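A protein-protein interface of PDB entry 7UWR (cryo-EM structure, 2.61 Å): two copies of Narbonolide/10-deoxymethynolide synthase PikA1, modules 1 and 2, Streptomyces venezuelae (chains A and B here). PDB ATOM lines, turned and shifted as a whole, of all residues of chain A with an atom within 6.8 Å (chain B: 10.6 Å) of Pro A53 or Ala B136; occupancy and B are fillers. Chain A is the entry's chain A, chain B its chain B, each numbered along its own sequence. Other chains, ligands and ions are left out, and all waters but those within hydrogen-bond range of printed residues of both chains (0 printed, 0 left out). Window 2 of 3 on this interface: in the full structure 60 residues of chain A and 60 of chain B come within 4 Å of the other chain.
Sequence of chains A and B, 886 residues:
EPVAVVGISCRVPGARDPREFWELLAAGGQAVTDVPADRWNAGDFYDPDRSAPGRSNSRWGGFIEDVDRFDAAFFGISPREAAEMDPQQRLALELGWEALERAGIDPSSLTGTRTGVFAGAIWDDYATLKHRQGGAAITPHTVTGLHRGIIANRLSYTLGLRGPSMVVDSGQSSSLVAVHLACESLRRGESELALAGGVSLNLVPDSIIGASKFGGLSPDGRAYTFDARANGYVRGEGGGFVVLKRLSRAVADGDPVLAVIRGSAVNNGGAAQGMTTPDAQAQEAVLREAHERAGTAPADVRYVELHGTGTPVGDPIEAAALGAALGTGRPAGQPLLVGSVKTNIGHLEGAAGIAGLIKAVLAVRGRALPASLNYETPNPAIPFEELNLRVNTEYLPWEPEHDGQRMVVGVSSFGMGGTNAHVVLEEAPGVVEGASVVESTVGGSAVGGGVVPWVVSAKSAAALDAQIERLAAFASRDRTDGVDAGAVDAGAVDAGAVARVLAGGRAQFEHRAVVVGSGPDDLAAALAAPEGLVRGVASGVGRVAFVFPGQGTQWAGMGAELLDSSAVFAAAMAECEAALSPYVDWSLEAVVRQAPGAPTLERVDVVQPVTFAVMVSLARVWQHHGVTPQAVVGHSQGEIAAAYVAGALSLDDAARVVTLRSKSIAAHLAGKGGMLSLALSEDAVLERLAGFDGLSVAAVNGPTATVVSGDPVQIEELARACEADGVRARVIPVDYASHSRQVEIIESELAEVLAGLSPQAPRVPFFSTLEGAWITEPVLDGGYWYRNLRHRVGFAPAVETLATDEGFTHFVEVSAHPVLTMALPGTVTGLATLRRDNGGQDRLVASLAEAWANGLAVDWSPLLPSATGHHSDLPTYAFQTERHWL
The side-chain amino group of Lys A213 sits at hydrogen-bond distance from the backbone carbonyl oxygen of Arg A50 (2.9 Å). The side-chain amino group of Lys A213 lies close to the backbone carbonyl oxygen of Ser A51, 3.5 Å away. O of Ala A52 is in hydrogen-bond range of NZ of Lys A213. OG1 of Thr B139 lies close to N of His B141 (3.1 Å). N of Thr B139 lies within hydrogen-bond range of OG1 of Thr B142.
Among the printed residues, merely in contact across the chains: Lys A213 with Pro B140, Gly A54 with Ala B136, Lys A213 with Thr B139, Lys A213 with Ile B138, Pro A53 with Ala B136 and Ile A209 with Ile B138.
No residue of chain B comes within 4 Å of Ser A51. No residue of chain B comes within 4 Å of Ala A52. Pro A53 touches just one residue of chain B: Ala B136. Printed residues of chain B within 4 Å of Gly A54: Ala B136. Glu B84 touches none of the printed residues of chain A. Ala B136 touches two residues of chain A. Of the printed residues of chain A, Ile B138 touches Ile A209 and Lys A213. Of the printed residues of chain A, Pro B140 touches Lys A213. The nearest residue of chain B that does not touch Pro A53 is Gly B135 (5.9 Å).
Hydrophobic or aromatic side chains of chain B within 4 Å of the printed part of chain A: Ala B136, Ile B138 and Pro B140. Printed residues of chain A that touch a printed residue of chain B: Pro A53, Gly A54, Ile A209 and Lys A213. Hydrophobic or aromatic side chains of chain A within 4 Å of the printed part of chain B: Pro A53 and Ile A209.
No position is printed for both chains. Of the 6 pairs that touch across the chains among the printed residues, none has its exchanged pair printed and touching as well.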
ATOM      1  N   ASP A  47      30.262  10.588  13.896  1.00  0.00           N
ATOM      2  CA  ASP A  47      29.833  10.429  15.276  1.00  0.00           C
ATOM      3  C   ASP A  47      30.832   9.500  15.953  1.00  0.00           C
ATOM      4  O   ASP A  47      31.108   8.415  15.417  1.00  0.00           O
ATOM      5  CB  ASP A  47      28.416   9.852  15.364  1.00  0.00           C
ATOM      6  CG  ASP A  47      27.814   9.939  16.762  1.00  0.00           C
ATOM      7  OD1 ASP A  47      28.550   9.828  17.761  1.00  0.00           O
ATOM      8  OD2 ASP A  47      26.586  10.126  16.865  1.00  0.00           O
ATOM      9  N   ASP A  49      30.289   7.605  18.381  1.00  0.00           N
ATOM     10  CA  ASP A  49      29.591   6.357  18.678  1.00  0.00           C
ATOM     11  C   ASP A  49      29.501   5.515  17.410  1.00  0.00           C
ATOM     12  O   ASP A  49      28.824   5.891  16.447  1.00  0.00           O
ATOM     13  CB  ASP A  49      28.207   6.656  19.248  1.00  0.00           C
ATOM     14  CG  ASP A  49      27.463   5.405  19.697  1.00  0.00           C
ATOM     15  OD1 ASP A  49      27.864   4.281  19.338  1.00  0.00           O
ATOM     16  OD2 ASP A  49      26.462   5.554  20.428  1.00  0.00           O
ATOM     17  N   ARG A  50      30.194   4.372  17.418  1.00  0.00           N
ATOM     18  CA  ARG A  50      30.149   3.426  16.305  1.00  0.00           C
ATOM     19  C   ARG A  50      28.730   2.981  15.969  1.00  0.00           C
ATOM     20  O   ARG A  50      28.437   2.671  14.809  1.00  0.00           O
ATOM     21  CB  ARG A  50      30.999   2.199  16.633  1.00  0.00           C
ATOM     22  CG  ARG A  50      32.492   2.448  16.718  1.00  0.00           C
ATOM     23  CD  ARG A  50      33.213   1.176  17.146  1.00  0.00           C
ATOM     24  NE  ARG A  50      34.663   1.315  17.109  1.00  0.00           N
ATOM     25  CZ  ARG A  50      35.442   0.817  16.159  1.00  0.00           C
ATOM     26  NH1 ARG A  50      34.934   0.218  15.093  1.00  0.00           N
ATOM     27  NH2 ARG A  50      36.759   0.952  16.263  1.00  0.00           N
ATOM     28  N   SER A  51      27.842   2.936  16.960  1.00  0.00           N
ATOM     29  CA  SER A  51      26.461   2.524  16.743  1.00  0.00           C
ATOM     30  C   SER A  51      25.587   3.602  16.116  1.00  0.00           C
ATOM     31  O   SER A  51      24.448   3.301  15.742  1.00  0.00           O
ATOM     32  CB  SER A  51      25.836   2.072  18.065  1.00  0.00           C
ATOM     33  OG  SER A  51      25.547   3.183  18.895  1.00  0.00           O
ATOM     34  N   ALA A  52      26.065   4.836  16.011  1.00  0.00           N
ATOM     35  CA  ALA A  52      25.202   5.923  15.569  1.00  0.00           C
ATOM     36  C   ALA A  52      24.744   5.685  14.133  1.00  0.00           C
ATOM     37  O   ALA A  52      25.565   5.325  13.277  1.00  0.00           O
ATOM     38  CB  ALA A  52      25.930   7.258  15.675  1.00  0.00           C
ATOM     39  N   PRO A  53      23.459   5.871  13.833  1.00  0.00           N
ATOM     40  CA  PRO A  53      22.935   5.473  12.520  1.00  0.00           C
ATOM     41  C   PRO A  53      23.447   6.378  11.406  1.00  0.00           C
ATOM     42  O   PRO A  53      23.418   7.606  11.518  1.00  0.00           O
ATOM     43  CB  PRO A  53      21.417   5.594  12.692  1.00  0.00           C
ATOM     44  CG  PRO A  53      21.245   6.619  13.760  1.00  0.00           C
ATOM     45  CD  PRO A  53      22.414   6.437  14.699  1.00  0.00           C
ATOM     46  N   GLY A  54      23.917   5.756  10.329  1.00  0.00           N
ATOM     47  CA  GLY A  54      24.299   6.476   9.133  1.00  0.00           C
ATOM     48  C   GLY A  54      25.507   7.372   9.269  1.00  0.00           C
ATOM     49  O   GLY A  54      25.682   8.282   8.457  1.00  0.00           O
ATOM     50  N   ARG A  55      26.341   7.149  10.278  1.00  0.00           N
ATOM     51  CA  ARG A  55      27.477   8.011  10.550  1.00  0.00           C
ATOM     52  C   ARG A  55      28.702   7.148  10.818  1.00  0.00           C
ATOM     53  O   ARG A  55      28.589   5.975  11.177  1.00  0.00           O
ATOM     54  CB  ARG A  55      27.180   8.965  11.720  1.00  0.00           C
ATOM     55  CG  ARG A  55      26.111   9.988  11.361  1.00  0.00           C
ATOM     56  CD  ARG A  55      26.075  11.196  12.280  1.00  0.00           C
ATOM     57  NE  ARG A  55      25.369  10.911  13.523  1.00  0.00           N
ATOM     58  CZ  ARG A  55      25.429  11.660  14.614  1.00  0.00           C
ATOM     59  NH1 ARG A  55      26.322  12.627  14.739  1.00  0.00           N
ATOM     60  NH2 ARG A  55      24.618  11.389  15.632  1.00  0.00           N
ATOM     61  N   SER A  56      29.882   7.734  10.628  1.00  0.00           N
ATOM     62  CA  SER A  56      31.135   7.005  10.768  1.00  0.00           C
ATOM     63  C   SER A  56      31.969   7.573  11.910  1.00  0.00           C
ATOM     64  O   SER A  56      31.946   8.776  12.183  1.00  0.00           O
ATOM     65  CB  SER A  56      31.939   7.055   9.460  1.00  0.00           C
ATOM     66  OG  SER A  56      33.065   6.197   9.501  1.00  0.00           O
ATOM     67  N   ILE A 209      30.691   4.657   5.812  1.00  0.00           N
ATOM     68  CA  ILE A 209      29.704   4.185   6.773  1.00  0.00           C
ATOM     69  C   ILE A 209      29.733   2.666   6.839  1.00  0.00           C
ATOM     70  O   ILE A 209      29.752   2.082   7.925  1.00  0.00           O
ATOM     71  CB  ILE A 209      28.305   4.713   6.412  1.00  0.00           C
ATOM     72  CG1 ILE A 209      28.300   6.240   6.430  1.00  0.00           C
ATOM     73  CG2 ILE A 209      27.270   4.180   7.380  1.00  0.00           C
ATOM     74  CD1 ILE A 209      27.222   6.844   5.578  1.00  0.00           C
ATOM     75  N   LYS A 213      30.553   0.447  10.084  1.00  0.00           N
ATOM     76  CA  LYS A 213      29.634  -0.531  10.655  1.00  0.00           C
ATOM     77  C   LYS A 213      30.239  -1.927  10.668  1.00  0.00           C
ATOM     78  O   LYS A 213      30.077  -2.668  11.643  1.00  0.00           O
ATOM     79  CB  LYS A 213      28.311  -0.522   9.887  1.00  0.00           C
ATOM     80  CG  LYS A 213      27.559   0.796   9.956  1.00  0.00           C
ATOM     81  CD  LYS A 213      27.368   1.253  11.389  1.00  0.00           C
ATOM     82  CE  LYS A 213      26.665   2.601  11.451  1.00  0.00           C
ATOM     83  NZ  LYS A 213      26.383   3.027  12.851  1.00  0.00           N
ATOM     84  N   GLU B  84      20.335  -8.845   4.588  1.00  0.00           N
ATOM     85  CA  GLU B  84      21.295  -7.965   3.926  1.00  0.00           C
ATOM     86  C   GLU B  84      21.954  -8.608   2.706  1.00  0.00           C
ATOM     87  O   GLU B  84      22.486  -7.891   1.854  1.00  0.00           O
ATOM     88  CB  GLU B  84      22.370  -7.530   4.920  1.00  0.00           C
ATOM     89  CG  GLU B  84      21.920  -6.460   5.895  1.00  0.00           C
ATOM     90  CD  GLU B  84      21.557  -5.156   5.215  1.00  0.00           C
ATOM     91  OE1 GLU B  84      22.463  -4.499   4.664  1.00  0.00           O
ATOM     92  OE2 GLU B  84      20.363  -4.789   5.233  1.00  0.00           O
ATOM     93  N   LEU B 129      19.120  -1.254  -4.495  1.00  0.00           N
ATOM     94  CA  LEU B 129      18.117  -1.125  -3.439  1.00  0.00           C
ATOM     95  C   LEU B 129      18.705  -0.605  -2.129  1.00  0.00           C
ATOM     96  O   LEU B 129      18.162   0.326  -1.525  1.00  0.00           O
ATOM     97  CB  LEU B 129      17.437  -2.474  -3.221  1.00  0.00           C
ATOM     98  CG  LEU B 129      16.542  -2.974  -4.355  1.00  0.00           C
ATOM     99  CD1 LEU B 129      16.317  -4.471  -4.232  1.00  0.00           C
ATOM    100  CD2 LEU B 129      15.217  -2.229  -4.351  1.00  0.00           C
ATOM    101  N   LYS B 130      19.807  -1.199  -1.662  1.00  0.00           N
ATOM    102  CA  LYS B 130      20.484  -0.686  -0.469  1.00  0.00           C
ATOM    103  C   LYS B 130      20.889   0.777  -0.602  1.00  0.00           C
ATOM    104  O   LYS B 130      20.819   1.536   0.370  1.00  0.00           O
ATOM    105  CB  LYS B 130      21.717  -1.534  -0.158  1.00  0.00           C
ATOM    106  CG  LYS B 130      21.437  -2.839   0.553  1.00  0.00           C
ATOM    107  CD  LYS B 130      20.638  -2.618   1.831  1.00  0.00           C
ATOM    108  CE  LYS B 130      21.271  -1.563   2.734  1.00  0.00           C
ATOM    109  NZ  LYS B 130      20.514  -1.393   4.004  1.00  0.00           N
ATOM    110  N   HIS B 131      21.327   1.189  -1.789  1.00  0.00           N
ATOM    111  CA  HIS B 131      21.701   2.580  -2.006  1.00  0.00           C
ATOM    112  C   HIS B 131      20.492   3.504  -1.959  1.00  0.00           C
ATOM    113  O   HIS B 131      20.521   4.542  -1.290  1.00  0.00           O
ATOM    114  CB  HIS B 131      22.423   2.712  -3.347  1.00  0.00           C
ATOM    115  CG  HIS B 131      23.686   1.913  -3.433  1.00  0.00           C
ATOM    116  ND1 HIS B 131      24.200   1.219  -2.360  1.00  0.00           N
ATOM    117  CD2 HIS B 131      24.510   1.659  -4.475  1.00  0.00           C
ATOM    118  CE1 HIS B 131      25.304   0.595  -2.732  1.00  0.00           C
ATOM    119  NE2 HIS B 131      25.513   0.847  -4.009  1.00  0.00           N
ATOM    120  N   ARG B 132      19.430   3.094  -2.662  1.00  0.00           N
ATOM    121  CA  ARG B 132      18.156   3.859  -2.693  1.00  0.00           C
ATOM    122  C   ARG B 132      17.693   4.065  -1.247  1.00  0.00           C
ATOM    123  O   ARG B 132      17.242   5.182  -0.925  1.00  0.00           O
ATOM    124  CB  ARG B 132      17.102   3.111  -3.515  1.00  0.00           C
ATOM    125  CG  ARG B 132      17.452   2.968  -4.990  1.00  0.00           C
ATOM    126  CD  ARG B 132      16.445   3.653  -5.893  1.00  0.00           C
ATOM    127  NE  ARG B 132      15.716   2.707  -6.726  1.00  0.00           N
ATOM    128  CZ  ARG B 132      14.714   1.946  -6.300  1.00  0.00           C
ATOM    129  NH1 ARG B 132      14.316   2.020  -5.041  1.00  0.00           N
ATOM    130  NH2 ARG B 132      14.113   1.115  -7.133  1.00  0.00           N
ATOM    131  N   GLN B 133      17.801   3.021  -0.416  1.00  0.00           N
ATOM    132  CA  GLN B 133      17.413   3.146   0.986  1.00  0.00           C
ATOM    133  C   GLN B 133      18.149   4.272   1.702  1.00  0.00           C
ATOM    134  O   GLN B 133      17.694   4.717   2.762  1.00  0.00           O
ATOM    135  CB  GLN B 133      17.638   1.821   1.716  1.00  0.00           C
ATOM    136  CG  GLN B 133      16.628   0.743   1.347  1.00  0.00           C
ATOM    137  CD  GLN B 133      16.785  -0.519   2.171  1.00  0.00           C
ATOM    138  OE1 GLN B 133      17.872  -1.088   2.256  1.00  0.00           O
ATOM    139  NE2 GLN B 133      15.694  -0.963   2.784  1.00  0.00           N
ATOM    140  N   GLY B 134      19.267   4.738   1.154  1.00  0.00           N
ATOM    141  CA  GLY B 134      20.007   5.856   1.703  1.00  0.00           C
ATOM    142  C   GLY B 134      20.805   5.545   2.964  1.00  0.00           C
ATOM    143  O   GLY B 134      21.129   4.399   3.284  1.00  0.00           O
ATOM    144  N   GLY B 135      21.123   6.621   3.682  1.00  0.00           N
ATOM    145  CA  GLY B 135      21.830   6.503   4.942  1.00  0.00           C
ATOM    146  C   GLY B 135      21.041   5.771   6.012  1.00  0.00           C
ATOM    147  O   GLY B 135      19.826   5.576   5.921  1.00  0.00           O
ATOM    148  N   ALA B 136      21.781   5.345   7.038  1.00  0.00           N
ATOM    149  CA  ALA B 136      21.287   4.650   8.226  1.00  0.00           C
ATOM    150  C   ALA B 136      20.708   3.268   7.953  1.00  0.00           C
ATOM    151  O   ALA B 136      20.579   2.461   8.878  1.00  0.00           O
ATOM    152  CB  ALA B 136      20.243   5.508   8.946  1.00  0.00           C
ATOM    153  N   ALA B 137      20.354   2.974   6.703  1.00  0.00           N
ATOM    154  CA  ALA B 137      20.053   1.597   6.337  1.00  0.00           C
ATOM    155  C   ALA B 137      21.300   0.724   6.275  1.00  0.00           C
ATOM    156  O   ALA B 137      21.178  -0.504   6.270  1.00  0.00           O
ATOM    157  CB  ALA B 137      19.319   1.558   4.997  1.00  0.00           C
ATOM    158  N   ILE B 138      22.489   1.323   6.224  1.00  0.00           N
ATOM    159  CA  ILE B 138      23.728   0.555   6.186  1.00  0.00           C
ATOM    160  C   ILE B 138      24.008  -0.072   7.546  1.00  0.00           C
ATOM    161  O   ILE B 138      23.969   0.603   8.581  1.00  0.00           O
ATOM    162  CB  ILE B 138      24.898   1.437   5.728  1.00  0.00           C
ATOM    163  CG1 ILE B 138      24.624   2.010   4.337  1.00  0.00           C
ATOM    164  CG2 ILE B 138      26.170   0.631   5.710  1.00  0.00           C
ATOM    165  CD1 ILE B 138      25.694   2.965   3.834  1.00  0.00           C
ATOM    166  N   THR B 139      24.301  -1.367   7.546  1.00  0.00           N
ATOM    167  CA  THR B 139      24.468  -2.177   8.744  1.00  0.00           C
ATOM    168  C   THR B 139      25.801  -2.905   8.659  1.00  0.00           C
ATOM    169  O   THR B 139      26.477  -2.864   7.627  1.00  0.00           O
ATOM    170  CB  THR B 139      23.310  -3.189   8.877  1.00  0.00           C
ATOM    171  OG1 THR B 139      23.592  -4.356   8.093  1.00  0.00           O
ATOM    172  CG2 THR B 139      21.993  -2.593   8.437  1.00  0.00           C
ATOM    173  N   PRO B 140      26.215  -3.593   9.731  1.00  0.00           N
ATOM    174  CA  PRO B 140      27.466  -4.374   9.669  1.00  0.00           C
ATOM    175  C   PRO B 140      27.474  -5.487   8.629  1.00  0.00           C
ATOM    176  O   PRO B 140      28.542  -6.060   8.385  1.00  0.00           O
ATOM    177  CB  PRO B 140      27.613  -4.928  11.095  1.00  0.00           C
ATOM    178  CG  PRO B 140      26.857  -3.966  11.931  1.00  0.00           C
ATOM    179  CD  PRO B 140      25.672  -3.597  11.102  1.00  0.00           C
ATOM    180  N   HIS B 141      26.333  -5.819   8.026  1.00  0.00           N
ATOM    181  CA  HIS B 141      26.259  -6.843   6.994  1.00  0.00           C
ATOM    182  C   HIS B 141      26.092  -6.287   5.588  1.00  0.00           C
ATOM    183  O   HIS B 141      26.118  -7.065   4.630  1.00  0.00           O
ATOM    184  CB  HIS B 141      25.106  -7.815   7.285  1.00  0.00           C
ATOM    185  CG  HIS B 141      25.296  -8.624   8.527  1.00  0.00           C
ATOM    186  ND1 HIS B 141      26.322  -9.532   8.672  1.00  0.00           N
ATOM    187  CD2 HIS B 141      24.590  -8.665   9.682  1.00  0.00           C
ATOM    188  CE1 HIS B 141      26.242 -10.095   9.864  1.00  0.00           C
ATOM    189  NE2 HIS B 141      25.200  -9.587  10.497  1.00  0.00           N
ATOM    190  N   THR B 142      25.905  -4.975   5.441  1.00  0.00           N
ATOM    191  CA  THR B 142      25.671  -4.388   4.124  1.00  0.00           C
ATOM    192  C   THR B 142      26.846  -4.627   3.180  1.00  0.00           C
ATOM    193  O   THR B 142      26.658  -5.052   2.038  1.00  0.00           O
ATOM    194  CB  THR B 142      25.401  -2.890   4.265  1.00  0.00           C
ATOM    195  OG1 THR B 142      24.304  -2.682   5.161  1.00  0.00           O
ATOM    196  CG2 THR B 142      25.072  -2.275   2.914  1.00  0.00           C
